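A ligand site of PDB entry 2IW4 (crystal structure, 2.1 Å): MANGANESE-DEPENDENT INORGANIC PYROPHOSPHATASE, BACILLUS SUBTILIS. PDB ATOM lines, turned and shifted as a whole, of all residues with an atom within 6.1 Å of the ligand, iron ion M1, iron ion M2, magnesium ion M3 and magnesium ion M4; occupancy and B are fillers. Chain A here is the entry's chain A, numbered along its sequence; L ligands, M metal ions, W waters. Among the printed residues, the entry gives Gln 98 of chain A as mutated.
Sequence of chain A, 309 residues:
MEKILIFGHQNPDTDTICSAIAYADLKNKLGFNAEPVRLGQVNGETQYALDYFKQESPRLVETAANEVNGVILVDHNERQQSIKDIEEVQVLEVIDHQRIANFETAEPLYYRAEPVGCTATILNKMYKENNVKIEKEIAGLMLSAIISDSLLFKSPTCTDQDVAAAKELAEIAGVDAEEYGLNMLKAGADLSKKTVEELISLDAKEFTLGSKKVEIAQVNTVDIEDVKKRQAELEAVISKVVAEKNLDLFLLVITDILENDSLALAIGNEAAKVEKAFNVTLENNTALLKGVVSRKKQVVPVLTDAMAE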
ATOM      1  N   HIS A   9      17.488  22.256  -4.634  1.00  0.00           N
ATOM      2  CA  HIS A   9      18.278  21.368  -3.792  1.00  0.00           C
ATOM      3  C   HIS A   9      18.419  19.936  -4.316  1.00  0.00           C
ATOM      4  O   HIS A   9      17.689  19.501  -5.226  1.00  0.00           O
ATOM      5  CB  HIS A   9      17.732  21.353  -2.356  1.00  0.00           C
ATOM      6  CG  HIS A   9      16.257  21.172  -2.271  1.00  0.00           C
ATOM      7  ND1 HIS A   9      15.645  19.933  -2.370  1.00  0.00           N
ATOM      8  CD2 HIS A   9      15.255  22.070  -2.080  1.00  0.00           C
ATOM      9  CE1 HIS A   9      14.325  20.085  -2.250  1.00  0.00           C
ATOM     10  NE2 HIS A   9      14.083  21.367  -2.077  1.00  0.00           N
ATOM     11  N   ASP A  13      12.320  18.408  -4.946  1.00  0.00           N
ATOM     12  CA  ASP A  13      10.871  18.331  -4.890  1.00  0.00           C
ATOM     13  C   ASP A  13      10.214  19.145  -6.004  1.00  0.00           C
ATOM     14  O   ASP A  13      10.897  19.694  -6.865  1.00  0.00           O
ATOM     15  CB  ASP A  13      10.329  18.734  -3.520  1.00  0.00           C
ATOM     16  CG  ASP A  13      10.936  20.003  -3.023  1.00  0.00           C
ATOM     17  OD1 ASP A  13      11.047  20.174  -1.784  1.00  0.00           O
ATOM     18  OD2 ASP A  13      11.309  20.855  -3.843  1.00  0.00           O
ATOM     19  N   THR A  14       8.889  19.212  -5.996  1.00  0.00           N
ATOM     20  CA  THR A  14       8.152  19.874  -7.066  1.00  0.00           C
ATOM     21  C   THR A  14       8.494  21.372  -7.126  1.00  0.00           C
ATOM     22  O   THR A  14       8.695  21.927  -8.212  1.00  0.00           O
ATOM     23  CB  THR A  14       6.640  19.620  -6.879  1.00  0.00           C
ATOM     24  OG1 THR A  14       6.431  18.198  -6.882  1.00  0.00           O
ATOM     25  CG2 THR A  14       5.825  20.252  -7.986  1.00  0.00           C
ATOM     26  N   ASP A  15       8.627  22.011  -5.969  1.00  0.00           N
ATOM     27  CA  ASP A  15       9.021  23.434  -5.932  1.00  0.00           C
ATOM     28  C   ASP A  15      10.426  23.615  -6.526  1.00  0.00           C
ATOM     29  O   ASP A  15      10.616  24.465  -7.371  1.00  0.00           O
ATOM     30  CB  ASP A  15       8.964  23.977  -4.499  1.00  0.00           C
ATOM     31  CG  ASP A  15       9.118  25.490  -4.410  1.00  0.00           C
ATOM     32  OD1 ASP A  15       8.849  26.217  -5.385  1.00  0.00           O
ATOM     33  OD2 ASP A  15       9.479  25.998  -3.321  1.00  0.00           O
ATOM     34  N   THR A  16      11.377  22.769  -6.122  1.00  0.00           N
ATOM     35  CA  THR A  16      12.746  22.828  -6.646  1.00  0.00           C
ATOM     36  C   THR A  16      12.846  22.638  -8.190  1.00  0.00           C
ATOM     37  O   THR A  16      13.624  23.329  -8.890  1.00  0.00           O
ATOM     38  CB  THR A  16      13.659  21.863  -5.875  1.00  0.00           C
ATOM     39  OG1 THR A  16      14.334  22.574  -4.832  1.00  0.00           O
ATOM     40  CG2 THR A  16      14.678  21.260  -6.729  1.00  0.00           C
ATOM     41  N   ASP A  75      14.991  27.840  -4.009  1.00  0.00           N
ATOM     42  CA  ASP A  75      14.411  26.892  -3.044  1.00  0.00           C
ATOM     43  C   ASP A  75      15.440  26.264  -2.090  1.00  0.00           C
ATOM     44  O   ASP A  75      15.138  25.285  -1.346  1.00  0.00           O
ATOM     45  CB  ASP A  75      13.608  25.817  -3.787  1.00  0.00           C
ATOM     46  CG  ASP A  75      12.807  24.957  -2.881  1.00  0.00           C
ATOM     47  OD1 ASP A  75      12.864  23.723  -3.047  1.00  0.00           O
ATOM     48  OD2 ASP A  75      12.111  25.508  -1.978  1.00  0.00           O
ATOM     49  N   ASP A  96      14.363  32.141  -2.495  1.00  0.00           N
ATOM     50  CA  ASP A  96      14.216  31.024  -1.547  1.00  0.00           C
ATOM     51  C   ASP A  96      13.202  31.326  -0.436  1.00  0.00           C
ATOM     52  O   ASP A  96      12.686  32.438  -0.337  1.00  0.00           O
ATOM     53  CB  ASP A  96      15.606  30.688  -0.961  1.00  0.00           C
ATOM     54  CG  ASP A  96      15.612  29.396  -0.121  1.00  0.00           C
ATOM     55  OD1 ASP A  96      16.427  29.273   0.813  1.00  0.00           O
ATOM     56  OD2 ASP A  96      14.754  28.524  -0.354  1.00  0.00           O
ATOM     57  N   HIS A  97      12.897  30.326   0.400  1.00  0.00           N
ATOM     58  CA  HIS A  97      12.002  30.528   1.531  1.00  0.00           C
ATOM     59  C   HIS A  97      12.344  29.611   2.701  1.00  0.00           C
ATOM     60  O   HIS A  97      11.472  29.324   3.529  1.00  0.00           O
ATOM     61  CB  HIS A  97      10.530  30.404   1.088  1.00  0.00           C
ATOM     62  CG  HIS A  97      10.126  29.036   0.622  1.00  0.00           C
ATOM     63  ND1 HIS A  97       8.938  28.446   1.011  1.00  0.00           N
ATOM     64  CD2 HIS A  97      10.716  28.153  -0.234  1.00  0.00           C
ATOM     65  CE1 HIS A  97       8.835  27.254   0.454  1.00  0.00           C
ATOM     66  NE2 HIS A  97       9.899  27.053  -0.312  1.00  0.00           N
ATOM     67  N   GLN A  98      13.615  29.149   2.756  1.00  0.00           N
ATOM     68  CA  GLN A  98      14.140  28.395   3.887  1.00  0.00           C
ATOM     69  C   GLN A  98      14.883  29.317   4.816  1.00  0.00           C
ATOM     70  O   GLN A  98      15.196  30.463   4.461  1.00  0.00           O
ATOM     71  CB  GLN A  98      15.152  27.315   3.447  1.00  0.00           C
ATOM     72  CG  GLN A  98      14.896  26.605   2.088  1.00  0.00           C
ATOM     73  CD  GLN A  98      13.601  25.831   2.016  1.00  0.00           C
ATOM     74  OE1 GLN A  98      13.162  25.214   2.986  1.00  0.00           O
ATOM     75  NE2 GLN A  98      12.993  25.827   0.831  1.00  0.00           N
ATOM     76  N   GLY A 117       4.950  30.349   1.791  1.00  0.00           N
ATOM     77  CA  GLY A 117       4.787  28.905   1.686  1.00  0.00           C
ATOM     78  C   GLY A 117       5.483  28.203   0.521  1.00  0.00           C
ATOM     79  O   GLY A 117       5.664  26.979   0.566  1.00  0.00           O
ATOM     80  N   CYS A 118       5.884  28.934  -0.522  1.00  0.00           N
ATOM     81  CA  CYS A 118       6.443  28.296  -1.721  1.00  0.00           C
ATOM     82  C   CYS A 118       7.369  29.276  -2.447  1.00  0.00           C
ATOM     83  O   CYS A 118       7.051  30.452  -2.517  1.00  0.00           O
ATOM     84  CB  CYS A 118       5.299  27.880  -2.650  1.00  0.00           C
ATOM     85  SG  CYS A 118       5.886  26.935  -4.024  1.00  0.00           S
ATOM     86  N   THR A 119       8.484  28.802  -3.018  1.00  0.00           N
ATOM     87  CA  THR A 119       9.376  29.670  -3.788  1.00  0.00           C
ATOM     88  C   THR A 119       8.647  30.276  -4.987  1.00  0.00           C
ATOM     89  O   THR A 119       8.868  31.440  -5.345  1.00  0.00           O
ATOM     90  CB  THR A 119      10.594  28.909  -4.359  1.00  0.00           C
ATOM     91  OG1 THR A 119      11.305  28.280  -3.286  1.00  0.00           O
ATOM     92  CG2 THR A 119      11.591  29.862  -5.089  1.00  0.00           C
ATOM     93  N   ALA A 145       3.896  23.556  -7.633  1.00  0.00           N
ATOM     94  CA  ALA A 145       4.854  23.862  -6.579  1.00  0.00           C
ATOM     95  C   ALA A 145       4.142  24.328  -5.287  1.00  0.00           C
ATOM     96  O   ALA A 145       4.427  23.824  -4.198  1.00  0.00           O
ATOM     97  CB  ALA A 145       5.858  24.897  -7.062  1.00  0.00           C
ATOM     98  N   SER A 148       2.163  21.506  -3.655  1.00  0.00           N
ATOM     99  CA  SER A 148       3.148  20.599  -3.093  1.00  0.00           C
ATOM    100  C   SER A 148       3.685  21.065  -1.764  1.00  0.00           C
ATOM    101  O   SER A 148       3.623  20.320  -0.797  1.00  0.00           O
ATOM    102  CB  SER A 148       4.331  20.434  -4.043  1.00  0.00           C
ATOM    103  OG  SER A 148       5.270  19.560  -3.461  1.00  0.00           O
ATOM    104  N   ASP A 149       4.242  22.282  -1.729  1.00  0.00           N
ATOM    105  CA  ASP A 149       4.805  22.878  -0.499  1.00  0.00           C
ATOM    106  C   ASP A 149       3.783  23.211   0.568  1.00  0.00           C
ATOM    107  O   ASP A 149       4.096  23.172   1.752  1.00  0.00           O
ATOM    108  CB  ASP A 149       5.539  24.174  -0.834  1.00  0.00           C
ATOM    109  CG  ASP A 149       6.959  23.936  -1.188  1.00  0.00           C
ATOM    110  OD1 ASP A 149       7.302  22.765  -1.441  1.00  0.00           O
ATOM    111  OD2 ASP A 149       7.757  24.888  -1.176  1.00  0.00           O
ATOM    112  N   THR A 157       2.950  26.761   6.825  1.00  0.00           N
ATOM    113  CA  THR A 157       3.788  27.695   6.062  1.00  0.00           C
ATOM    114  C   THR A 157       2.967  28.505   5.034  1.00  0.00           C
ATOM    115  O   THR A 157       3.444  29.517   4.522  1.00  0.00           O
ATOM    116  CB  THR A 157       4.877  26.979   5.292  1.00  0.00           C
ATOM    117  OG1 THR A 157       4.252  26.008   4.448  1.00  0.00           O
ATOM    118  CG2 THR A 157       5.822  26.300   6.259  1.00  0.00           C
ATOM    119  N   ASP A 203      13.078  12.769  -0.055  1.00  0.00           N
ATOM    120  CA  ASP A 203      12.911  14.123   0.450  1.00  0.00           C
ATOM    121  C   ASP A 203      13.805  14.276   1.681  1.00  0.00           C
ATOM    122  O   ASP A 203      13.355  14.673   2.782  1.00  0.00           O
ATOM    123  CB  ASP A 203      11.432  14.366   0.748  1.00  0.00           C
ATOM    124  CG  ASP A 203      11.106  15.810   1.093  1.00  0.00           C
ATOM    125  OD1 ASP A 203      11.920  16.701   0.845  1.00  0.00           O
ATOM    126  OD2 ASP A 203       9.990  16.049   1.606  1.00  0.00           O
ATOM    127  N   LYS A 205      17.123  16.066   3.594  1.00  0.00           N
ATOM    128  CA  LYS A 205      17.958  17.276   3.679  1.00  0.00           C
ATOM    129  C   LYS A 205      18.915  17.173   4.852  1.00  0.00           C
ATOM    130  O   LYS A 205      18.522  16.783   5.939  1.00  0.00           O
ATOM    131  CB  LYS A 205      17.100  18.515   3.865  1.00  0.00           C
ATOM    132  CG  LYS A 205      16.443  19.006   2.602  1.00  0.00           C
ATOM    133  CD  LYS A 205      15.504  20.118   2.881  1.00  0.00           C
ATOM    134  CE  LYS A 205      14.763  20.559   1.631  1.00  0.00           C
ATOM    135  NZ  LYS A 205      14.122  21.911   1.823  1.00  0.00           N
ATOM    136  N   PHE A 207      21.437  19.128   7.576  1.00  0.00           N
ATOM    137  CA  PHE A 207      21.517  20.362   8.349  1.00  0.00           C
ATOM    138  C   PHE A 207      22.689  20.212   9.337  1.00  0.00           C
ATOM    139  O   PHE A 207      23.085  19.091   9.681  1.00  0.00           O
ATOM    140  CB  PHE A 207      20.228  20.592   9.151  1.00  0.00           C
ATOM    141  CG  PHE A 207      19.034  20.796   8.295  1.00  0.00           C
ATOM    142  CD1 PHE A 207      18.196  19.723   7.964  1.00  0.00           C
ATOM    143  CD2 PHE A 207      18.759  22.051   7.786  1.00  0.00           C
ATOM    144  CE1 PHE A 207      17.100  19.905   7.162  1.00  0.00           C
ATOM    145  CE2 PHE A 207      17.661  22.246   6.955  1.00  0.00           C
ATOM    146  CZ  PHE A 207      16.836  21.164   6.640  1.00  0.00           C
ATOM    147  N   GLN A 218      11.628  13.407   4.939  1.00  0.00           N
ATOM    148  CA  GLN A 218      10.181  13.402   5.062  1.00  0.00           C
ATOM    149  C   GLN A 218       9.543  12.490   3.990  1.00  0.00           C
ATOM    150  O   GLN A 218      10.092  12.356   2.883  1.00  0.00           O
ATOM    151  CB  GLN A 218       9.611  14.838   4.966  1.00  0.00           C
ATOM    152  CG  GLN A 218       8.118  14.968   5.149  1.00  0.00           C
ATOM    153  CD  GLN A 218       7.660  16.398   5.422  1.00  0.00           C
ATOM    154  OE1 GLN A 218       8.322  17.361   5.030  1.00  0.00           O
ATOM    155  NE2 GLN A 218       6.507  16.552   6.088  1.00  0.00           N
ATOM    156  N   SER A 294       5.487  20.599   8.640  1.00  0.00           N
ATOM    157  CA  SER A 294       6.451  21.452   7.974  1.00  0.00           C
ATOM    158  C   SER A 294       7.859  21.350   8.569  1.00  0.00           C
ATOM    159  O   SER A 294       8.019  21.572   9.773  1.00  0.00           O
ATOM    160  CB  SER A 294       5.993  22.906   8.083  1.00  0.00           C
ATOM    161  OG  SER A 294       7.111  23.721   7.757  1.00  0.00           O
ATOM    162  N   ARG A 295       8.860  20.984   7.756  1.00  0.00           N
ATOM    163  CA  ARG A 295      10.239  20.854   8.237  1.00  0.00           C
ATOM    164  C   ARG A 295      10.770  22.240   8.599  1.00  0.00           C
ATOM    165  O   ARG A 295      11.244  22.442   9.712  1.00  0.00           O
ATOM    166  CB  ARG A 295      11.168  20.205   7.187  1.00  0.00           C
ATOM    167  CG  ARG A 295      12.621  19.909   7.668  1.00  0.00           C
ATOM    168  CD  ARG A 295      13.328  18.914   6.695  1.00  0.00           C
ATOM    169  NE  ARG A 295      12.842  19.142   5.332  1.00  0.00           N
ATOM    170  CZ  ARG A 295      12.810  18.231   4.357  1.00  0.00           C
ATOM    171  NH1 ARG A 295      13.289  17.012   4.574  1.00  0.00           N
ATOM    172  NH2 ARG A 295      12.328  18.544   3.137  1.00  0.00           N
ATOM    173  N   LYS A 296      10.637  23.190   7.652  1.00  0.00           N
ATOM    174  CA  LYS A 296      11.214  24.529   7.801  1.00  0.00           C
ATOM    175  C   LYS A 296      10.677  25.288   8.998  1.00  0.00           C
ATOM    176  O   LYS A 296      11.389  26.107   9.566  1.00  0.00           O
ATOM    177  CB  LYS A 296      11.076  25.407   6.535  1.00  0.00           C
ATOM    178  CG  LYS A 296       9.654  25.893   6.263  1.00  0.00           C
ATOM    179  CD  LYS A 296       9.544  26.850   5.079  1.00  0.00           C
ATOM    180  CE  LYS A 296      10.225  26.283   3.828  1.00  0.00           C
ATOM    181  NZ  LYS A 296       9.448  25.188   3.149  1.00  0.00           N
ATOM    182  N   LYS A 297       9.406  25.044   9.363  1.00  0.00           N
ATOM    183  CA  LYS A 297       8.715  25.852  10.358  1.00  0.00           C
ATOM    184  C   LYS A 297       8.518  25.084  11.665  1.00  0.00           C
ATOM    185  O   LYS A 297       8.580  25.651  12.753  1.00  0.00           O
ATOM    186  CB  LYS A 297       7.363  26.335   9.791  1.00  0.00           C
ATOM    187  CG  LYS A 297       6.448  27.061  10.832  1.00  0.00           C
ATOM    188  CD  LYS A 297       5.294  27.782  10.163  1.00  0.00           C
ATOM    189  CE  LYS A 297       4.451  28.554  11.140  1.00  0.00           C
ATOM    190  NZ  LYS A 297       4.825  29.978  11.003  1.00  0.00           N
ATOM    191  N   VAL A 300      12.898  22.129  12.035  1.00  0.00           N
ATOM    192  CA  VAL A 300      14.232  22.725  12.198  1.00  0.00           C
ATOM    193  C   VAL A 300      14.358  23.692  13.391  1.00  0.00           C
ATOM    194  O   VAL A 300      15.306  23.544  14.156  1.00  0.00           O
ATOM    195  CB  VAL A 300      14.829  23.348  10.880  1.00  0.00           C
ATOM    196  CG1 VAL A 300      16.126  24.159  11.201  1.00  0.00           C
ATOM    197  CG2 VAL A 300      15.103  22.251   9.836  1.00  0.00           C
HETATM  198  P1  LIG L   1      10.843  22.878   0.943  1.00  0.00           P
HETATM  199  O1  LIG L   1      10.403  24.317   0.622  1.00  0.00           O
HETATM  200  O2  LIG L   1       9.684  21.930   0.937  1.00  0.00           O
HETATM  201  O3  LIG L   1      12.103  22.507   0.195  1.00  0.00           O
HETATM  202  N1  LIG L   1      11.353  22.906   2.540  1.00  0.00           N
HETATM  203  P2  LIG L   1      11.026  21.935   3.863  1.00  0.00           P
HETATM  204  O4  LIG L   1      10.046  22.621   4.850  1.00  0.00           O
HETATM  205  O5  LIG L   1      10.368  20.642   3.376  1.00  0.00           O
HETATM  206  O6  LIG L   1      12.446  21.763   4.483  1.00  0.00           O
HETATM  207 FE    FE M   1      12.002  22.276  -1.819  1.00  0.00          FE
HETATM  208 FE    FE M   2      10.006  25.009  -1.434  1.00  0.00          FE
HETATM  209 MG    MG M   3       9.276  20.172   1.640  1.00  0.00          MG
HETATM  210 MG    MG M   4       8.744  21.260  -1.177  1.00  0.00          MG
HETATM  211  O   HOH W   1       7.688  20.923  -3.498  1.00  0.00           O
HETATM  212  O   HOH W   2       7.943  19.607   0.057  1.00  0.00           O
HETATM  213  O   HOH W   3      10.001  22.753  -1.986  1.00  0.00           O
HETATM  214  O   HOH W   4      14.021  23.847   5.171  1.00  0.00           O
HETATM  215  O   HOH W   5       7.443  23.294   1.857  1.00  0.00           O
HETATM  216  O   HOH W   6       7.610  20.630   2.612  1.00  0.00           O
HETATM  217  O   HOH W   7      10.775  19.229   0.776  1.00  0.00           O
HETATM  218  O   HOH W   8       7.401  23.349   5.143  1.00  0.00           O
HETATM  219  O   HOH W   9       8.917  18.280   2.567  1.00  0.00           O
HETATM  220  O   HOH W  10       8.385  20.058   5.105  1.00  0.00           O
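Iron ion M1 is bound by O3 of the ligand (2.0 Å).
Iron ion M1 is bound by water W3, at 2.1 Å.
OD1 of Asp 75 is bound to iron ion M1.
NE2 of His 9 is bound to iron ion M1.
OD1 of Asp 13 binds iron ion M1, 2.3 Å away.
OD2 of Asp 13 is bound to iron ion M1, 2.6 Å away.
Residues that only touch iron ion M2: Gln 98 (3.8 Å) and Thr 119 (3.98 Å).
Water W9 lies within hydrogen-bond range of the side-chain carboxylate of Asp 203, the side-chain amide oxygen of Gln 218 and the guanidinium group of Arg 295.
Water W7 lies within hydrogen-bond range of the side-chain carboxylate of Asp 203 (2.8 Å) and the guanidinium group of Arg 295 (2.9 Å).
Water W10 lies within hydrogen-bond range of the side-chain amide oxygen of Gln 218 (2.7 Å), the backbone NH of Arg 295 (2.8 Å) and an oxygen (O4) of the ligand (3.1 Å).
Water W4 lies within hydrogen-bond range of an oxygen (O6) of the ligand (2.7 Å) and the side-chain amide oxygen (OE1) of Gln 98 (2.7 Å).
Water W8 lies within hydrogen-bond range of OG of Ser 294 (2.7 Å), O4 of the ligand (2.8 Å) and NZ of Lys 296 (3.4 Å).
Water W5 lies within hydrogen-bond range of the side-chain amino group of Lys 296 and the backbone carbonyl oxygen of Asp 149.
Arg 295 touches magnesium ion M3.
The nearest printed residue that does not touch the ligand is Gln 218 (4.2 Å).
Iron ion M2 is bound by the side-chain carboxylate of Asp 15 (2.2 Å), an oxygen (O1) of the ligand (2.2 Å), the side-chain carboxylate of Asp 75 (2.2 Å), the side-chain carboxylate of Asp 149 (2.3 Å), water W3 (2.3 Å) and a ring nitrogen (NE2) of His 97 (2.3 Å).
Iron ion M2 has six donor atoms within binding distance.
The backbone carbonyl oxygen of Asp 75 is in hydrogen-bond range of the side-chain amide nitrogen of Gln 98, 3.1 Å away.
The side-chain carboxylate of Asp 15 sits close to the side-chain hydroxyl of Thr 119 (2.9 Å).
N of Gln 98 lies close to OD2 of Asp 96 (3.4 Å).
OD1 of Asp 15 sits at hydrogen-bond distance from SG of Cys 118.
The backbone NH (N) of His 9 lies close to the side-chain hydroxyl (OG1) of Thr 16.
The backbone carbonyl oxygen of Arg 295 lies within hydrogen-bond range of the backbone NH of Val 300 (2.9 Å).
The side-chain hydroxyl (OG1) of Thr 119 sits close to the side-chain carboxylate (OD2) of Asp 75 (3.2 Å).
OD1 of Asp 75 lies close to OG1 of Thr 16, at 2.6 Å.
Magnesium ion M4 is bound by OD1 of Asp 149 (2.1 Å), water W3 (2.1 Å), water W2 (2.2 Å), O2 of the ligand (2.4 Å) and water W1 (2.6 Å).
Slightly farther from magnesium ion M4 lies OD1 of Asp 13 (2.6 Å).
Merely in contact with iron ion M1: Thr 16 (3.8 Å).
Within 4 Å of iron ion M1: His 9, Asp 13, Thr 16 and Asp 75.
O4 of the ligand sits at hydrogen-bond distance from N of Lys 296, 2.9 Å away.
An oxygen (O6) of the ligand is in salt-bridge range of the guanidinium group (NE) of Arg 295 (2.8 Å).
A nitrogen (N1) of the ligand is in hydrogen-bond range of the side-chain amide oxygen (OE1) of Gln 98, 3.0 Å away.
An oxygen (O4) of the ligand is in salt-bridge range of the side-chain amino group (NZ) of Lys 296 (3.1 Å).
An oxygen (O6) of the ligand is in salt-bridge range of the side-chain amino group (NZ) of Lys 205, at 3.1 Å.
Magnesium ion M3 is bound by O2 of the ligand (1.9 Å), water W7 (2.0 Å), water W6 (2.0 Å), O5 of the ligand (2.1 Å), water W9 (2.1 Å) and water W2 (2.1 Å).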
